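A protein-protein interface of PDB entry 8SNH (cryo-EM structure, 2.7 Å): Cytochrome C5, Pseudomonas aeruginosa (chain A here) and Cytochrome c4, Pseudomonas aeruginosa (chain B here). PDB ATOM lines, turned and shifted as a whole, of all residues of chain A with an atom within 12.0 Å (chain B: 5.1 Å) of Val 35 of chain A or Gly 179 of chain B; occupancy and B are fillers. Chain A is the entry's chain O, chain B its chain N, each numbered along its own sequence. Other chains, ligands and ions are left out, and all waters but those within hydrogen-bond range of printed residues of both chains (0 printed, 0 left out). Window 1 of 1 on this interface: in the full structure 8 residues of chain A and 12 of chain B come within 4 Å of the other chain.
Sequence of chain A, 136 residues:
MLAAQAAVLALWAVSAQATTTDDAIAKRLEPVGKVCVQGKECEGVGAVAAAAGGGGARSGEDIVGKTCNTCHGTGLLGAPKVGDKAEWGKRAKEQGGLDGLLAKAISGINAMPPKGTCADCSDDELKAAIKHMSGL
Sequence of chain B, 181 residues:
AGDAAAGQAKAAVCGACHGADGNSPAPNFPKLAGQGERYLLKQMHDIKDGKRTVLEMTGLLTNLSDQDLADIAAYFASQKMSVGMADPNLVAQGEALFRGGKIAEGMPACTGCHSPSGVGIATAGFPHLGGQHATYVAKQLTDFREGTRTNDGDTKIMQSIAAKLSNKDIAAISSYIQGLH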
ATOM      1  N   GLU A  30     -10.354  -5.172   5.538  1.00  0.00           N
ATOM      2  CA  GLU A  30     -10.102  -4.285   4.410  1.00  0.00           C
ATOM      3  C   GLU A  30      -9.374  -5.037   3.298  1.00  0.00           C
ATOM      4  O   GLU A  30      -8.369  -5.709   3.569  1.00  0.00           O
ATOM      5  CB  GLU A  30      -9.273  -3.083   4.860  1.00  0.00           C
ATOM      6  CG  GLU A  30      -9.390  -1.865   3.958  1.00  0.00           C
ATOM      7  CD  GLU A  30     -10.768  -1.234   3.996  1.00  0.00           C
ATOM      8  OE1 GLU A  30     -10.952  -0.246   4.738  1.00  0.00           O
ATOM      9  OE2 GLU A  30     -11.665  -1.720   3.276  1.00  0.00           O
ATOM     10  N   PRO A  31      -9.835  -4.956   2.047  1.00  0.00           N
ATOM     11  CA  PRO A  31      -9.122  -5.640   0.963  1.00  0.00           C
ATOM     12  C   PRO A  31      -7.704  -5.111   0.807  1.00  0.00           C
ATOM     13  O   PRO A  31      -7.428  -3.930   1.026  1.00  0.00           O
ATOM     14  CB  PRO A  31      -9.973  -5.337  -0.276  1.00  0.00           C
ATOM     15  CG  PRO A  31     -11.310  -4.970   0.253  1.00  0.00           C
ATOM     16  CD  PRO A  31     -11.053  -4.289   1.556  1.00  0.00           C
ATOM     17  N   VAL A  32      -6.797  -6.012   0.426  1.00  0.00           N
ATOM     18  CA  VAL A  32      -5.395  -5.638   0.271  1.00  0.00           C
ATOM     19  C   VAL A  32      -5.228  -4.653  -0.880  1.00  0.00           C
ATOM     20  O   VAL A  32      -4.518  -3.648  -0.759  1.00  0.00           O
ATOM     21  CB  VAL A  32      -4.529  -6.893   0.069  1.00  0.00           C
ATOM     22  CG1 VAL A  32      -3.121  -6.511  -0.369  1.00  0.00           C
ATOM     23  CG2 VAL A  32      -4.497  -7.720   1.342  1.00  0.00           C
ATOM     24  N   GLY A  33      -5.876  -4.925  -2.008  1.00  0.00           N
ATOM     25  CA  GLY A  33      -5.683  -4.114  -3.194  1.00  0.00           C
ATOM     26  C   GLY A  33      -6.333  -2.752  -3.048  1.00  0.00           C
ATOM     27  O   GLY A  33      -7.564  -2.658  -2.907  1.00  0.00           O
ATOM     28  N   LYS A  34      -5.531  -1.693  -3.081  1.00  0.00           N
ATOM     29  CA  LYS A  34      -6.022  -0.322  -3.061  1.00  0.00           C
ATOM     30  C   LYS A  34      -5.834   0.296  -4.440  1.00  0.00           C
ATOM     31  O   LYS A  34      -4.786   0.123  -5.068  1.00  0.00           O
ATOM     32  CB  LYS A  34      -5.289   0.511  -2.007  1.00  0.00           C
ATOM     33  CG  LYS A  34      -5.973   0.538  -0.648  1.00  0.00           C
ATOM     34  CD  LYS A  34      -5.083  -0.040   0.440  1.00  0.00           C
ATOM     35  CE  LYS A  34      -3.964   0.918   0.814  1.00  0.00           C
ATOM     36  NZ  LYS A  34      -2.911   0.257   1.634  1.00  0.00           N
ATOM     37  N   VAL A  35      -6.853   1.013  -4.907  1.00  0.00           N
ATOM     38  CA  VAL A  35      -6.882   1.564  -6.255  1.00  0.00           C
ATOM     39  C   VAL A  35      -7.063   3.072  -6.165  1.00  0.00           C
ATOM     40  O   VAL A  35      -7.964   3.555  -5.470  1.00  0.00           O
ATOM     41  CB  VAL A  35      -8.001   0.928  -7.102  1.00  0.00           C
ATOM     42  CG1 VAL A  35      -9.370   1.256  -6.526  1.00  0.00           C
ATOM     43  CG2 VAL A  35      -7.904   1.385  -8.553  1.00  0.00           C
ATOM     44  N   CYS A  36      -6.202   3.811  -6.860  1.00  0.00           N
ATOM     45  CA  CYS A  36      -6.378   5.247  -7.008  1.00  0.00           C
ATOM     46  C   CYS A  36      -7.345   5.532  -8.147  1.00  0.00           C
ATOM     47  O   CYS A  36      -7.268   4.917  -9.215  1.00  0.00           O
ATOM     48  CB  CYS A  36      -5.036   5.928  -7.278  1.00  0.00           C
ATOM     49  SG  CYS A  36      -3.822   5.737  -5.955  1.00  0.00           S
ATOM     50  N   VAL A  37      -8.261   6.469  -7.917  1.00  0.00           N
ATOM     51  CA  VAL A  37      -9.303   6.808  -8.876  1.00  0.00           C
ATOM     52  C   VAL A  37      -9.297   8.313  -9.092  1.00  0.00           C
ATOM     53  O   VAL A  37      -9.077   9.085  -8.152  1.00  0.00           O
ATOM     54  CB  VAL A  37     -10.690   6.329  -8.398  1.00  0.00           C
ATOM     55  CG1 VAL A  37     -11.764   6.729  -9.395  1.00  0.00           C
ATOM     56  CG2 VAL A  37     -10.687   4.825  -8.188  1.00  0.00           C
ATOM     57  N   GLN A  38      -9.533   8.729 -10.335  1.00  0.00           N
ATOM     58  CA  GLN A  38      -9.563  10.149 -10.656  1.00  0.00           C
ATOM     59  C   GLN A  38     -10.626  10.856  -9.824  1.00  0.00           C
ATOM     60  O   GLN A  38     -11.758  10.381  -9.706  1.00  0.00           O
ATOM     61  CB  GLN A  38      -9.842  10.347 -12.146  1.00  0.00           C
ATOM     62  CG  GLN A  38      -8.775   9.768 -13.061  1.00  0.00           C
ATOM     63  CD  GLN A  38      -9.209   9.734 -14.513  1.00  0.00           C
ATOM     64  OE1 GLN A  38     -10.338  10.098 -14.845  1.00  0.00           O
ATOM     65  NE2 GLN A  38      -8.314   9.292 -15.389  1.00  0.00           N
ATOM     66  N   GLY A  39     -10.254  11.993  -9.247  1.00  0.00           N
ATOM     67  CA  GLY A  39     -11.165  12.755  -8.414  1.00  0.00           C
ATOM     68  C   GLY A  39     -11.574  12.007  -7.161  1.00  0.00           C
ATOM     69  O   GLY A  39     -10.931  11.033  -6.769  1.00  0.00           O
ATOM     70  N   VAL B  83       2.215   5.121  -9.544  1.00  0.00           N
ATOM     71  CA  VAL B  83       0.819   4.702  -9.561  1.00  0.00           C
ATOM     72  C   VAL B  83      -0.003   5.780 -10.252  1.00  0.00           C
ATOM     73  O   VAL B  83       0.062   6.956  -9.876  1.00  0.00           O
ATOM     74  CB  VAL B  83       0.290   4.441  -8.140  1.00  0.00           C
ATOM     75  CG1 VAL B  83      -1.125   3.884  -8.194  1.00  0.00           C
ATOM     76  CG2 VAL B  83       1.215   3.489  -7.396  1.00  0.00           C
ATOM     77  N   GLY B  84      -0.770   5.378 -11.258  1.00  0.00           N
ATOM     78  CA  GLY B  84      -1.694   6.261 -11.935  1.00  0.00           C
ATOM     79  C   GLY B  84      -3.051   6.270 -11.265  1.00  0.00           C
ATOM     80  O   GLY B  84      -3.200   5.910 -10.094  1.00  0.00           O
ATOM     81  N   MET B  85      -4.057   6.688 -12.026  1.00  0.00           N
ATOM     82  CA  MET B  85      -5.427   6.766 -11.545  1.00  0.00           C
ATOM     83  C   MET B  85      -6.328   5.912 -12.425  1.00  0.00           C
ATOM     84  O   MET B  85      -6.098   5.790 -13.632  1.00  0.00           O
ATOM     85  CB  MET B  85      -5.935   8.212 -11.535  1.00  0.00           C
ATOM     86  CG  MET B  85      -4.909   9.237 -11.078  1.00  0.00           C
ATOM     87  SD  MET B  85      -5.575  10.432  -9.903  1.00  0.00           S
ATOM     88  CE  MET B  85      -5.927   9.379  -8.498  1.00  0.00           C
ATOM     89  N   ALA B  86      -7.349   5.325 -11.813  1.00  0.00           N
ATOM     90  CA  ALA B  86      -8.335   4.536 -12.534  1.00  0.00           C
ATOM     91  C   ALA B  86      -9.531   5.402 -12.908  1.00  0.00           C
ATOM     92  O   ALA B  86      -9.904   6.329 -12.186  1.00  0.00           O
ATOM     93  CB  ALA B  86      -8.797   3.346 -11.691  1.00  0.00           C
ATOM     94  N   VAL B  91     -13.672   1.664 -12.762  1.00  0.00           N
ATOM     95  CA  VAL B  91     -12.935   1.070 -11.652  1.00  0.00           C
ATOM     96  C   VAL B  91     -13.716  -0.084 -11.034  1.00  0.00           C
ATOM     97  O   VAL B  91     -13.127  -1.071 -10.587  1.00  0.00           O
ATOM     98  CB  VAL B  91     -12.585   2.144 -10.606  1.00  0.00           C
ATOM     99  CG1 VAL B  91     -13.816   2.541  -9.808  1.00  0.00           C
ATOM    100  CG2 VAL B  91     -11.481   1.640  -9.688  1.00  0.00           C
ATOM    101  N   GLU B  95     -12.055  -3.674 -11.056  1.00  0.00           N
ATOM    102  CA  GLU B  95     -11.756  -4.253  -9.753  1.00  0.00           C
ATOM    103  C   GLU B  95     -12.420  -5.612  -9.598  1.00  0.00           C
ATOM    104  O   GLU B  95     -11.801  -6.562  -9.103  1.00  0.00           O
ATOM    105  CB  GLU B  95     -12.218  -3.304  -8.648  1.00  0.00           C
ATOM    106  CG  GLU B  95     -12.009  -3.829  -7.242  1.00  0.00           C
ATOM    107  CD  GLU B  95     -12.397  -2.818  -6.184  1.00  0.00           C
ATOM    108  OE1 GLU B  95     -13.609  -2.594  -5.993  1.00  0.00           O
ATOM    109  OE2 GLU B  95     -11.489  -2.246  -5.546  1.00  0.00           O
ATOM    110  N   SER B 174      -7.669  -2.750 -17.253  1.00  0.00           N
ATOM    111  CA  SER B 174      -6.481  -1.931 -17.460  1.00  0.00           C
ATOM    112  C   SER B 174      -6.559  -0.642 -16.654  1.00  0.00           C
ATOM    113  O   SER B 174      -5.570  -0.224 -16.042  1.00  0.00           O
ATOM    114  CB  SER B 174      -6.313  -1.619 -18.947  1.00  0.00           C
ATOM    115  OG  SER B 174      -6.342  -2.802 -19.721  1.00  0.00           O
ATOM    116  N   SER B 175      -7.727   0.001 -16.639  1.00  0.00           N
ATOM    117  CA  SER B 175      -7.885   1.210 -15.838  1.00  0.00           C
ATOM    118  C   SER B 175      -7.667   0.912 -14.358  1.00  0.00           C
ATOM    119  O   SER B 175      -6.939   1.635 -13.663  1.00  0.00           O
ATOM    120  CB  SER B 175      -9.272   1.810 -16.071  1.00  0.00           C
ATOM    121  OG  SER B 175      -9.254   3.213 -15.889  1.00  0.00           O
ATOM    122  N   TYR B 176      -8.277  -0.168 -13.866  1.00  0.00           N
ATOM    123  CA  TYR B 176      -8.110  -0.532 -12.463  1.00  0.00           C
ATOM    124  C   TYR B 176      -6.650  -0.827 -12.141  1.00  0.00           C
ATOM    125  O   TYR B 176      -6.137  -0.400 -11.101  1.00  0.00           O
ATOM    126  CB  TYR B 176      -8.986  -1.737 -12.128  1.00  0.00           C
ATOM    127  CG  TYR B 176      -8.730  -2.308 -10.754  1.00  0.00           C
ATOM    128  CD1 TYR B 176      -9.266  -1.709  -9.624  1.00  0.00           C
ATOM    129  CD2 TYR B 176      -7.951  -3.443 -10.587  1.00  0.00           C
ATOM    130  CE1 TYR B 176      -9.034  -2.225  -8.367  1.00  0.00           C
ATOM    131  CE2 TYR B 176      -7.715  -3.966  -9.333  1.00  0.00           C
ATOM    132  CZ  TYR B 176      -8.258  -3.354  -8.227  1.00  0.00           C
ATOM    133  OH  TYR B 176      -8.026  -3.871  -6.974  1.00  0.00           O
ATOM    134  N   ILE B 177      -5.964  -1.554 -13.024  1.00  0.00           N
ATOM    135  CA  ILE B 177      -4.554  -1.864 -12.812  1.00  0.00           C
ATOM    136  C   ILE B 177      -3.737  -0.582 -12.766  1.00  0.00           C
ATOM    137  O   ILE B 177      -2.825  -0.438 -11.942  1.00  0.00           O
ATOM    138  CB  ILE B 177      -4.054  -2.819 -13.912  1.00  0.00           C
ATOM    139  CG1 ILE B 177      -4.557  -4.238 -13.647  1.00  0.00           C
ATOM    140  CG2 ILE B 177      -2.535  -2.804 -13.989  1.00  0.00           C
ATOM    141  CD1 ILE B 177      -4.564  -5.121 -14.874  1.00  0.00           C
ATOM    142  N   GLN B 178      -4.048   0.370 -13.645  1.00  0.00           N
ATOM    143  CA  GLN B 178      -3.347   1.646 -13.619  1.00  0.00           C
ATOM    144  C   GLN B 178      -3.539   2.339 -12.279  1.00  0.00           C
ATOM    145  O   GLN B 178      -2.587   2.885 -11.710  1.00  0.00           O
ATOM    146  CB  GLN B 178      -3.836   2.538 -14.758  1.00  0.00           C
ATOM    147  CG  GLN B 178      -3.227   3.928 -14.752  1.00  0.00           C
ATOM    148  CD  GLN B 178      -3.413   4.648 -16.069  1.00  0.00           C
ATOM    149  OE1 GLN B 178      -2.589   4.535 -16.973  1.00  0.00           O
ATOM    150  NE2 GLN B 178      -4.500   5.401 -16.182  1.00  0.00           N
ATOM    151  N   GLY B 179      -4.762   2.320 -11.753  1.00  0.00           N
ATOM    152  CA  GLY B 179      -4.996   2.891 -10.438  1.00  0.00           C
ATOM    153  C   GLY B 179      -4.560   2.027  -9.272  1.00  0.00           C
ATOM    154  O   GLY B 179      -4.492   2.522  -8.144  1.00  0.00           O
ATOM    155  N   LEU B 180      -4.250   0.757  -9.519  1.00  0.00           N
ATOM    156  CA  LEU B 180      -3.994  -0.187  -8.442  1.00  0.00           C
ATOM    157  C   LEU B 180      -2.634   0.060  -7.796  1.00  0.00           C
ATOM    158  O   LEU B 180      -1.676   0.484  -8.446  1.00  0.00           O
ATOM    159  CB  LEU B 180      -4.065  -1.618  -8.974  1.00  0.00           C
ATOM    160  CG  LEU B 180      -3.764  -2.752  -7.992  1.00  0.00           C
ATOM    161  CD1 LEU B 180      -4.802  -2.796  -6.887  1.00  0.00           C
ATOM    162  CD2 LEU B 180      -3.711  -4.078  -8.727  1.00  0.00           C
ATOM    163  N   HIS B 181      -2.562  -0.215  -6.496  1.00  0.00           N
ATOM    164  CA  HIS B 181      -1.303  -0.155  -5.759  1.00  0.00           C
ATOM    165  C   HIS B 181      -1.409  -0.954  -4.464  1.00  0.00           C
ATOM    166  O   HIS B 181      -2.502  -1.203  -3.958  1.00  0.00           O
ATOM    167  CB  HIS B 181      -0.914   1.291  -5.453  1.00  0.00           C
ATOM    168  CG  HIS B 181      -1.933   2.036  -4.649  1.00  0.00           C
ATOM    169  ND1 HIS B 181      -1.801   2.249  -3.294  1.00  0.00           N
ATOM    170  CD2 HIS B 181      -3.099   2.622  -5.010  1.00  0.00           C
ATOM    171  CE1 HIS B 181      -2.842   2.934  -2.854  1.00  0.00           C
ATOM    172  NE2 HIS B 181      -3.644   3.172  -3.876  1.00  0.00           N
ATOM    173  OXT HIS B 181      -0.403  -1.371  -3.892  1.00  0.00           O
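Glu 30 of chain A touches none of the printed residues of chain B. Printed residues of chain B within 4 Å of Lys 34 of chain A: Gly 179 (3.9 Å), Leu 180 (3.4 Å) and His 181 (2.7 Å). Of the printed residues of chain B, Val 35 of chain A touches Ala 86, Val 91, Tyr 176, Gly 179 and Leu 180. Printed residues of chain B within 4 Å of Cys 36 of chain A: Val 83, Gly 84, Met 85, Ala 86, Gly 179 and His 181. Printed residues of chain B within 4 Å of Gln 38 of chain A: Met 85 and Ala 86. Of chain A, only Cys 36 (3.96 Å) comes within 4 Å of Val 83 of chain B. Of chain A, only Cys 36 comes within 4 Å of Gly 84 of chain B. Met 85 of chain B touches just these residues of chain A: Cys 36 (3.5 Å), Val 37 (3.2 Å) and Gln 38 (3.6 Å). Of chain A, only Val 35 (3.8 Å), Cys 36 (2.6 Å), Val 37 (3.4 Å) and Gln 38 (3.1 Å) come within 4 Å of Ala 86 of chain B. Val 91 of chain B touches just these residues of chain A: Val 35 and Val 37. Tyr 176 of chain B touches just one residue of chain A: Val 35. No residue of chain A comes within 4 Å of Gln 178 of chain B. Of chain A, only Lys 34 (3.9 Å), Val 35 (3.2 Å) and Cys 36 (2.5 Å) come within 4 Å of Gly 179 of chain B. Of the printed residues of chain A, Leu 180 of chain B touches Lys 34 (3.4 Å) and Val 35 (3.8 Å).
Of the 14 printed residues of chain B, 9 touch a printed residue of chain A. Printed residues of chain B that touch a printed residue of chain A: Val 83, Gly 84, Met 85, Ala 86, Val 91, Tyr 176, Gly 179, Leu 180 and His 181. Hydrophobic or aromatic side chains of chain B that line the printed part of chain A: Val 83, Met 85, Ala 86, Val 91, Tyr 176, Leu 180 and His 181. Along chain B the printed residues that touch a printed residue of chain A span positions 83 to 181. Hydrophobic or aromatic side chains of chain A that line the printed part of chain B: Val 35 and Val 37. Among the printed residues, 19 pairs touch across the chains. Among the printed residues, no Asp or Glu carboxylate lies within 4 Å of a Lys or Arg side-chain nitrogen of the other chain.
NE2 of Gln 178 of chain B sits at hydrogen-bond distance from O of Met 85 of chain B (3.0 Å). N of Gly 84 of chain B is in hydrogen-bond range of O of Gln 178 of chain B (3.1 Å).
Among the printed residues, pairs that only touch across the chains: Lys 34 of chain A with Gly 179 of chain B (3.9 Å), Lys 34 of chain A with Leu 180 of chain B (3.4 Å), Val 35 of chain A with Ala 86 of chain B (3.8 Å), Val 35 of chain A with Val 91 of chain B (3.8 Å), Val 35 of chain A with Tyr 176 of chain B (3.5 Å), Val 35 of chain A with Gly 179 of chain B (3.2 Å), Val 35 of chain A with Leu 180 of chain B (3.8 Å), Cys 36 of chain A with Val 83 of chain B (3.96 Å), Cys 36 of chain A with Gly 84 of chain B (3.4 Å), Cys 36 of chain A with Met 85 of chain B (3.5 Å), Val 37 of chain A with Met 85 of chain B (3.2 Å), Val 37 of chain A with Ala 86 of chain B (3.4 Å), Val 37 of chain A with Val 91 of chain B (3.6 Å) and Gln 38 of chain A with Met 85 of chain B (3.6 Å).
NE2 of His 181 of chain B lies within hydrogen-bond range of SG of Cys 36 of chain A, 3.3 Å away. The backbone carbonyl oxygen of Ala 86 of chain B lies within hydrogen-bond range of the backbone NH of Gln 38 of chain A, 3.1 Å away. N of Cys 36 of chain A is in hydrogen-bond range of O of Gly 179 of chain B (2.5 Å). The backbone carbonyl oxygen of Lys 34 of chain A sits at hydrogen-bond distance from the backbone NH of His 181 of chain B (2.7 Å). O of Cys 36 of chain A is in hydrogen-bond range of N of Ala 86 of chain B (2.6 Å).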
